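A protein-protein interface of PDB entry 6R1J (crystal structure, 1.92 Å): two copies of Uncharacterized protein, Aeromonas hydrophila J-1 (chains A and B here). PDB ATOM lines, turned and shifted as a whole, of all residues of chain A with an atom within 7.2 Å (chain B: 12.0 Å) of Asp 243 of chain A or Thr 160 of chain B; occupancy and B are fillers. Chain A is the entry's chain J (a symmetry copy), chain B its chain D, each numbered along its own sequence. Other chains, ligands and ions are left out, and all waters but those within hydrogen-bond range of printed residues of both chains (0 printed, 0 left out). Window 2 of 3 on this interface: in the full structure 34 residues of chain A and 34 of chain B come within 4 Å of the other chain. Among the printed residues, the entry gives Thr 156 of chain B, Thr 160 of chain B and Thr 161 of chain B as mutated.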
ATOM      1  N   PHE A  76      -3.116   3.695  -7.098  1.00  0.00           N
ATOM      2  CA  PHE A  76      -3.536   4.758  -6.148  1.00  0.00           C
ATOM      3  C   PHE A  76      -4.818   4.259  -5.445  1.00  0.00           C
ATOM      4  O   PHE A  76      -5.776   3.891  -6.159  1.00  0.00           O
ATOM      5  CB  PHE A  76      -3.712   6.119  -6.840  1.00  0.00           C
ATOM      6  CG  PHE A  76      -2.447   6.843  -7.254  1.00  0.00           C
ATOM      7  CD1 PHE A  76      -1.722   7.588  -6.334  1.00  0.00           C
ATOM      8  CD2 PHE A  76      -2.016   6.827  -8.580  1.00  0.00           C
ATOM      9  CE1 PHE A  76      -0.570   8.265  -6.722  1.00  0.00           C
ATOM     10  CE2 PHE A  76      -0.872   7.508  -8.969  1.00  0.00           C
ATOM     11  CZ  PHE A  76      -0.156   8.229  -8.039  1.00  0.00           C
ATOM     12  N   LEU A  81      -6.207   9.205  -2.343  1.00  0.00           N
ATOM     13  CA  LEU A  81      -6.330  10.279  -3.362  1.00  0.00           C
ATOM     14  C   LEU A  81      -7.236  11.380  -2.807  1.00  0.00           C
ATOM     15  O   LEU A  81      -6.800  12.521  -2.748  1.00  0.00           O
ATOM     16  CB  LEU A  81      -6.977   9.783  -4.661  1.00  0.00           C
ATOM     17  CG  LEU A  81      -6.104   9.089  -5.696  1.00  0.00           C
ATOM     18  CD1 LEU A  81      -6.885   8.967  -6.991  1.00  0.00           C
ATOM     19  CD2 LEU A  81      -4.802   9.842  -5.939  1.00  0.00           C
ATOM     20  N   ASP A 238     -12.449  11.197 -10.123  1.00  0.00           N
ATOM     21  CA  ASP A 238     -12.307   9.712 -10.062  1.00  0.00           C
ATOM     22  C   ASP A 238     -13.079   9.186  -8.843  1.00  0.00           C
ATOM     23  O   ASP A 238     -13.981   8.341  -9.039  1.00  0.00           O
ATOM     24  CB  ASP A 238     -10.837   9.277  -9.972  1.00  0.00           C
ATOM     25  CG  ASP A 238     -10.011   9.497 -11.235  1.00  0.00           C
ATOM     26  OD1 ASP A 238     -10.622   9.799 -12.287  1.00  0.00           O
ATOM     27  OD2 ASP A 238      -8.757   9.356 -11.166  1.00  0.00           O
ATOM     28  N   ASP A 243      -8.917   5.506 -12.130  1.00  0.00           N
ATOM     29  CA  ASP A 243      -7.753   4.901 -12.831  1.00  0.00           C
ATOM     30  C   ASP A 243      -6.463   5.538 -12.293  1.00  0.00           C
ATOM     31  O   ASP A 243      -6.333   6.765 -12.273  1.00  0.00           O
ATOM     32  CB  ASP A 243      -7.930   5.023 -14.352  1.00  0.00           C
ATOM     33  CG  ASP A 243      -6.811   4.393 -15.168  1.00  0.00           C
ATOM     34  OD1 ASP A 243      -6.002   3.675 -14.570  1.00  0.00           O
ATOM     35  OD2 ASP A 243      -6.741   4.645 -16.396  1.00  0.00           O
ATOM     36  N   PRO A 244      -5.501   4.733 -11.769  1.00  0.00           N
ATOM     37  CA  PRO A 244      -4.204   5.242 -11.293  1.00  0.00           C
ATOM     38  C   PRO A 244      -3.339   6.037 -12.288  1.00  0.00           C
ATOM     39  O   PRO A 244      -2.473   6.784 -11.844  1.00  0.00           O
ATOM     40  CB  PRO A 244      -3.424   3.966 -10.925  1.00  0.00           C
ATOM     41  CG  PRO A 244      -4.502   2.982 -10.543  1.00  0.00           C
ATOM     42  CD  PRO A 244      -5.655   3.296 -11.478  1.00  0.00           C
ATOM     43  N   GLU A 245      -3.548   5.844 -13.593  1.00  0.00           N
ATOM     44  CA  GLU A 245      -2.798   6.557 -14.664  1.00  0.00           C
ATOM     45  C   GLU A 245      -3.398   7.962 -14.865  1.00  0.00           C
ATOM     46  O   GLU A 245      -2.664   8.852 -15.371  1.00  0.00           O
ATOM     47  CB  GLU A 245      -2.825   5.718 -15.945  1.00  0.00           C
ATOM     48  CG  GLU A 245      -1.793   6.108 -16.996  1.00  0.00           C
ATOM     49  CD  GLU A 245      -0.383   5.583 -16.771  1.00  0.00           C
ATOM     50  OE1 GLU A 245       0.019   5.425 -15.592  1.00  0.00           O
ATOM     51  OE2 GLU A 245       0.307   5.306 -17.779  1.00  0.00           O
ATOM     52  N   LEU A 246      -4.687   8.159 -14.540  1.00  0.00           N
ATOM     53  CA  LEU A 246      -5.350   9.488 -14.670  1.00  0.00           C
ATOM     54  C   LEU A 246      -4.866  10.368 -13.532  1.00  0.00           C
ATOM     55  O   LEU A 246      -4.492  11.509 -13.788  1.00  0.00           O
ATOM     56  CB  LEU A 246      -6.876   9.384 -14.669  1.00  0.00           C
ATOM     57  CG  LEU A 246      -7.490   9.201 -16.054  1.00  0.00           C
ATOM     58  CD1 LEU A 246      -9.001   9.098 -15.945  1.00  0.00           C
ATOM     59  CD2 LEU A 246      -7.088  10.338 -16.994  1.00  0.00           C
ATOM     60  N   ALA A 247      -4.835   9.822 -12.330  1.00  0.00           N
ATOM     61  CA  ALA A 247      -4.311  10.542 -11.173  1.00  0.00           C
ATOM     62  C   ALA A 247      -2.887  10.994 -11.537  1.00  0.00           C
ATOM     63  O   ALA A 247      -2.577  12.148 -11.284  1.00  0.00           O
ATOM     64  CB  ALA A 247      -4.383   9.671  -9.957  1.00  0.00           C
ATOM     65  N   ARG A 248      -2.097  10.150 -12.212  1.00  0.00           N
ATOM     66  CA  ARG A 248      -0.687  10.448 -12.562  1.00  0.00           C
ATOM     67  C   ARG A 248      -0.669  11.595 -13.583  1.00  0.00           C
ATOM     68  O   ARG A 248       0.190  12.482 -13.475  1.00  0.00           O
ATOM     69  CB  ARG A 248      -0.007   9.160 -13.045  1.00  0.00           C
ATOM     70  CG  ARG A 248       1.467   9.284 -13.398  1.00  0.00           C
ATOM     71  CD  ARG A 248       2.102   7.913 -13.681  1.00  0.00           C
ATOM     72  NE  ARG A 248       1.941   7.120 -12.474  1.00  0.00           N
ATOM     73  CZ  ARG A 248       2.741   7.212 -11.416  1.00  0.00           C
ATOM     74  NH1 ARG A 248       3.778   8.035 -11.445  1.00  0.00           N
ATOM     75  NH2 ARG A 248       2.511   6.479 -10.341  1.00  0.00           N
ATOM     76  N   LEU A 249      -1.586  11.585 -14.549  1.00  0.00           N
ATOM     77  CA  LEU A 249      -1.681  12.645 -15.585  1.00  0.00           C
ATOM     78  C   LEU A 249      -1.942  14.001 -14.929  1.00  0.00           C
ATOM     79  O   LEU A 249      -1.180  14.939 -15.231  1.00  0.00           O
ATOM     80  CB  LEU A 249      -2.786  12.321 -16.583  1.00  0.00           C
ATOM     81  CG  LEU A 249      -2.940  13.311 -17.737  1.00  0.00           C
ATOM     82  CD1 LEU A 249      -1.890  13.051 -18.811  1.00  0.00           C
ATOM     83  CD2 LEU A 249      -4.340  13.227 -18.320  1.00  0.00           C
ATOM     84  N   LYS B 151       0.672  22.845 -26.087  1.00  0.00           N
ATOM     85  CA  LYS B 151       0.912  21.376 -26.072  1.00  0.00           C
ATOM     86  C   LYS B 151       0.517  20.791 -24.715  1.00  0.00           C
ATOM     87  O   LYS B 151      -0.077  19.718 -24.719  1.00  0.00           O
ATOM     88  CB  LYS B 151       2.339  21.031 -26.473  1.00  0.00           C
ATOM     89  CG  LYS B 151       2.606  21.281 -27.940  1.00  0.00           C
ATOM     90  CD  LYS B 151       3.989  20.925 -28.370  1.00  0.00           C
ATOM     91  CE  LYS B 151       4.291  21.478 -29.743  1.00  0.00           C
ATOM     92  NZ  LYS B 151       5.669  21.129 -30.151  1.00  0.00           N
ATOM     93  N   LYS B 152       0.776  21.499 -23.621  1.00  0.00           N
ATOM     94  CA  LYS B 152       0.448  21.059 -22.241  1.00  0.00           C
ATOM     95  C   LYS B 152      -1.072  20.880 -22.143  1.00  0.00           C
ATOM     96  O   LYS B 152      -1.516  19.837 -21.633  1.00  0.00           O
ATOM     97  CB  LYS B 152       1.023  22.066 -21.232  1.00  0.00           C
ATOM     98  CG  LYS B 152       0.913  21.737 -19.745  1.00  0.00           C
ATOM     99  CD  LYS B 152      -0.343  22.297 -19.060  1.00  0.00           C
ATOM    100  CE  LYS B 152      -0.446  21.954 -17.582  1.00  0.00           C
ATOM    101  NZ  LYS B 152      -1.794  22.155 -16.978  1.00  0.00           N
ATOM    102  N   LEU B 153      -1.854  21.844 -22.634  1.00  0.00           N
ATOM    103  CA  LEU B 153      -3.336  21.802 -22.483  1.00  0.00           C
ATOM    104  C   LEU B 153      -3.897  20.652 -23.326  1.00  0.00           C
ATOM    105  O   LEU B 153      -4.717  19.877 -22.816  1.00  0.00           O
ATOM    106  CB  LEU B 153      -3.896  23.185 -22.834  1.00  0.00           C
ATOM    107  CG  LEU B 153      -3.457  24.272 -21.860  1.00  0.00           C
ATOM    108  CD1 LEU B 153      -3.749  25.658 -22.411  1.00  0.00           C
ATOM    109  CD2 LEU B 153      -4.101  24.071 -20.493  1.00  0.00           C
ATOM    110  N   TYR B 154      -3.373  20.493 -24.527  1.00  0.00           N
ATOM    111  CA  TYR B 154      -3.718  19.417 -25.481  1.00  0.00           C
ATOM    112  C   TYR B 154      -3.415  18.032 -24.890  1.00  0.00           C
ATOM    113  O   TYR B 154      -4.357  17.194 -24.799  1.00  0.00           O
ATOM    114  CB  TYR B 154      -2.935  19.678 -26.761  1.00  0.00           C
ATOM    115  CG  TYR B 154      -3.087  18.630 -27.821  1.00  0.00           C
ATOM    116  CD1 TYR B 154      -4.155  18.684 -28.702  1.00  0.00           C
ATOM    117  CD2 TYR B 154      -2.165  17.603 -27.961  1.00  0.00           C
ATOM    118  CE1 TYR B 154      -4.313  17.734 -29.698  1.00  0.00           C
ATOM    119  CE2 TYR B 154      -2.310  16.646 -28.954  1.00  0.00           C
ATOM    120  CZ  TYR B 154      -3.391  16.712 -29.823  1.00  0.00           C
ATOM    121  OH  TYR B 154      -3.561  15.797 -30.824  1.00  0.00           O
ATOM    122  N   LEU B 155      -2.166  17.790 -24.446  1.00  0.00           N
ATOM    123  CA  LEU B 155      -1.746  16.458 -23.933  1.00  0.00           C
ATOM    124  C   LEU B 155      -2.607  16.052 -22.739  1.00  0.00           C
ATOM    125  O   LEU B 155      -3.042  14.892 -22.690  1.00  0.00           O
ATOM    126  CB  LEU B 155      -0.255  16.464 -23.587  1.00  0.00           C
ATOM    127  CG  LEU B 155       0.678  16.452 -24.796  1.00  0.00           C
ATOM    128  CD1 LEU B 155       2.110  16.751 -24.383  1.00  0.00           C
ATOM    129  CD2 LEU B 155       0.584  15.131 -25.553  1.00  0.00           C
ATOM    130  N   THR B 156      -2.892  17.002 -21.862  1.00  0.00           N
ATOM    131  CA  THR B 156      -3.698  16.800 -20.639  1.00  0.00           C
ATOM    132  C   THR B 156      -5.122  16.413 -21.047  1.00  0.00           C
ATOM    133  O   THR B 156      -5.734  15.608 -20.335  1.00  0.00           O
ATOM    134  CB  THR B 156      -3.615  18.043 -19.750  1.00  0.00           C
ATOM    135  OG1 THR B 156      -2.230  18.278 -19.467  1.00  0.00           O
ATOM    136  CG2 THR B 156      -4.391  17.885 -18.470  1.00  0.00           C
ATOM    137  N   GLY B 157      -5.598  16.958 -22.172  1.00  0.00           N
ATOM    138  CA  GLY B 157      -6.923  16.647 -22.733  1.00  0.00           C
ATOM    139  C   GLY B 157      -6.972  15.253 -23.351  1.00  0.00           C
ATOM    140  O   GLY B 157      -8.077  14.746 -23.510  1.00  0.00           O
ATOM    141  N   LEU B 158      -5.835  14.650 -23.715  1.00  0.00           N
ATOM    142  CA  LEU B 158      -5.814  13.305 -24.347  1.00  0.00           C
ATOM    143  C   LEU B 158      -6.010  12.191 -23.306  1.00  0.00           C
ATOM    144  O   LEU B 158      -5.910  11.052 -23.708  1.00  0.00           O
ATOM    145  CB  LEU B 158      -4.484  13.060 -25.059  1.00  0.00           C
ATOM    146  CG  LEU B 158      -4.215  13.850 -26.325  1.00  0.00           C
ATOM    147  CD1 LEU B 158      -2.983  13.282 -27.015  1.00  0.00           C
ATOM    148  CD2 LEU B 158      -5.421  13.804 -27.252  1.00  0.00           C
ATOM    149  N   GLY B 159      -6.216  12.467 -22.017  1.00  0.00           N
ATOM    150  CA  GLY B 159      -6.270  11.385 -21.012  1.00  0.00           C
ATOM    151  C   GLY B 159      -4.909  10.691 -20.902  1.00  0.00           C
ATOM    152  O   GLY B 159      -3.912  11.341 -21.219  1.00  0.00           O
ATOM    153  N   THR B 160      -4.870   9.401 -20.545  1.00  0.00           N
ATOM    154  CA  THR B 160      -3.630   8.622 -20.241  1.00  0.00           C
ATOM    155  C   THR B 160      -2.717   8.529 -21.458  1.00  0.00           C
ATOM    156  O   THR B 160      -1.504   8.386 -21.250  1.00  0.00           O
ATOM    157  CB  THR B 160      -3.929   7.210 -19.712  1.00  0.00           C
ATOM    158  OG1 THR B 160      -4.574   6.478 -20.750  1.00  0.00           O
ATOM    159  CG2 THR B 160      -4.795   7.218 -18.474  1.00  0.00           C
ATOM    160  N   THR B 161      -3.258   8.594 -22.678  1.00  0.00           N
ATOM    161  CA  THR B 161      -2.456   8.576 -23.925  1.00  0.00           C
ATOM    162  C   THR B 161      -1.460   9.755 -23.894  1.00  0.00           C
ATOM    163  O   THR B 161      -0.353   9.584 -24.405  1.00  0.00           O
ATOM    164  CB  THR B 161      -3.322   8.641 -25.196  1.00  0.00           C
ATOM    165  OG1 THR B 161      -4.177   7.504 -25.266  1.00  0.00           O
ATOM    166  CG2 THR B 161      -2.507   8.663 -26.471  1.00  0.00           C
ATOM    167  N   GLY B 162      -1.825  10.884 -23.275  1.00  0.00           N
ATOM    168  CA  GLY B 162      -0.982  12.094 -23.215  1.00  0.00           C
ATOM    169  C   GLY B 162       0.081  12.087 -22.122  1.00  0.00           C
ATOM    170  O   GLY B 162       0.892  13.034 -22.110  1.00  0.00           O
ATOM    171  N   LEU B 163       0.146  11.083 -21.241  1.00  0.00           N
ATOM    172  CA  LEU B 163       1.066  11.144 -20.066  1.00  0.00           C
ATOM    173  C   LEU B 163       2.550  11.074 -20.457  1.00  0.00           C
ATOM    174  O   LEU B 163       3.340  11.898 -19.985  1.00  0.00           O
ATOM    175  CB  LEU B 163       0.676  10.086 -19.037  1.00  0.00           C
ATOM    176  CG  LEU B 163       1.663   9.916 -17.894  1.00  0.00           C
ATOM    177  CD1 LEU B 163       1.799  11.187 -17.058  1.00  0.00           C
ATOM    178  CD2 LEU B 163       1.249   8.730 -17.035  1.00  0.00           C
ATOM    179  N   PRO B 164       3.035  10.114 -21.277  1.00  0.00           N
ATOM    180  CA  PRO B 164       4.449  10.139 -21.674  1.00  0.00           C
ATOM    181  C   PRO B 164       4.831  11.494 -22.301  1.00  0.00           C
ATOM    182  O   PRO B 164       5.844  12.066 -21.935  1.00  0.00           O
ATOM    183  CB  PRO B 164       4.583   8.997 -22.695  1.00  0.00           C
ATOM    184  CG  PRO B 164       3.410   8.070 -22.367  1.00  0.00           C
ATOM    185  CD  PRO B 164       2.299   8.959 -21.825  1.00  0.00           C
ATOM    186  N   GLY B 165       3.986  12.004 -23.200  1.00  0.00           N
ATOM    187  CA  GLY B 165       4.186  13.289 -23.899  1.00  0.00           C
ATOM    188  C   GLY B 165       4.242  14.478 -22.938  1.00  0.00           C
ATOM    189  O   GLY B 165       5.038  15.389 -23.211  1.00  0.00           O
ATOM    190  N   LEU B 166       3.425  14.473 -21.870  1.00  0.00           N
ATOM    191  CA  LEU B 166       3.318  15.570 -20.874  1.00  0.00           C
ATOM    192  C   LEU B 166       4.575  15.548 -20.009  1.00  0.00           C
ATOM    193  O   LEU B 166       5.096  16.632 -19.682  1.00  0.00           O
ATOM    194  CB  LEU B 166       2.060  15.394 -20.014  1.00  0.00           C
ATOM    195  CG  LEU B 166       1.838  16.458 -18.947  1.00  0.00           C
ATOM    196  CD1 LEU B 166       1.690  17.836 -19.586  1.00  0.00           C
ATOM    197  CD2 LEU B 166       0.634  16.140 -18.082  1.00  0.00           C
ATOM    198  N   ILE B 167       5.011  14.351 -19.635  1.00  0.00           N
ATOM    199  CA  ILE B 167       6.233  14.155 -18.793  1.00  0.00           C
ATOM    200  C   ILE B 167       7.428  14.770 -19.529  1.00  0.00           C
ATOM    201  O   ILE B 167       8.182  15.504 -18.873  1.00  0.00           O
ATOM    202  CB  ILE B 167       6.461  12.671 -18.429  1.00  0.00           C
ATOM    203  CG1 ILE B 167       5.436  12.189 -17.396  1.00  0.00           C
ATOM    204  CG2 ILE B 167       7.902  12.441 -17.959  1.00  0.00           C
ATOM    205  CD1 ILE B 167       5.489  10.675 -17.110  1.00  0.00           C
ATOM    206  N   ALA B 168       7.606  14.455 -20.809  1.00  0.00           N
ATOM    207  CA  ALA B 168       8.715  14.962 -21.643  1.00  0.00           C
ATOM    208  C   ALA B 168       8.599  16.487 -21.786  1.00  0.00           C
ATOM    209  O   ALA B 168       9.621  17.187 -21.655  1.00  0.00           O
ATOM    210  CB  ALA B 168       8.699  14.290 -22.990  1.00  0.00           C
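No position is printed for both chains. Of the 9 pairs that touch across the chains among the printed residues, none has its exchanged pair printed and touching as well.
Among the printed residues, pairs that only touch across the chains: Asp 243 of chain A with Thr 160 of chain B (3.8 Å), Glu 245 of chain A with Thr 160 of chain B (3.5 Å), Glu 245 of chain A with Leu 163 of chain B (3.6 Å), Arg 248 of chain A with Leu 163 of chain B (3.6 Å), Leu 249 of chain A with Thr 156 of chain B (3.4 Å), Leu 249 of chain A with Gly 159 of chain B (3.5 Å), Leu 249 of chain A with Gly 162 of chain B (3.97 Å), Leu 249 of chain A with Leu 163 of chain B (3.7 Å) and Leu 249 of chain A with Leu 166 of chain B (3.6 Å).
Of the printed residues of chain B, Asp 243 of chain A touches Thr 160 (3.8 Å). No residue of chain B comes within 4 Å of Pro 244 of chain A. No residue of chain B comes within 4 Å of Leu 246 of chain A. Of the printed residues of chain A, Thr 156 of chain B touches Leu 249. Of the printed residues of chain A, Gly 159 of chain B touches Leu 249. Of the printed residues of chain A, Leu 163 of chain B touches Glu 245 (3.6 Å), Arg 248 (3.6 Å) and Leu 249 (3.7 Å). The nearest printed residue of chain A that does not touch Thr 156 of chain B is Leu 246 of chain A (6.4 Å).
Hydrophobic or aromatic side chains of chain B within 4 Å of the printed part of chain A: Leu 163 and Leu 166. Hydrophobic or aromatic side chains of chain A within 4 Å of the printed part of chain B: Leu 249. Among the printed residues, 9 pairs touch across the chains.
The backbone carbonyl oxygen (O) of Lys 152 of chain B is in hydrogen-bond range of the side-chain hydroxyl (OG1) of Thr 156 of chain B (2.8 Å). The side-chain carboxylate of Asp 243 of chain A sits close to the backbone NH of Glu 245 of chain A (3.4 Å).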
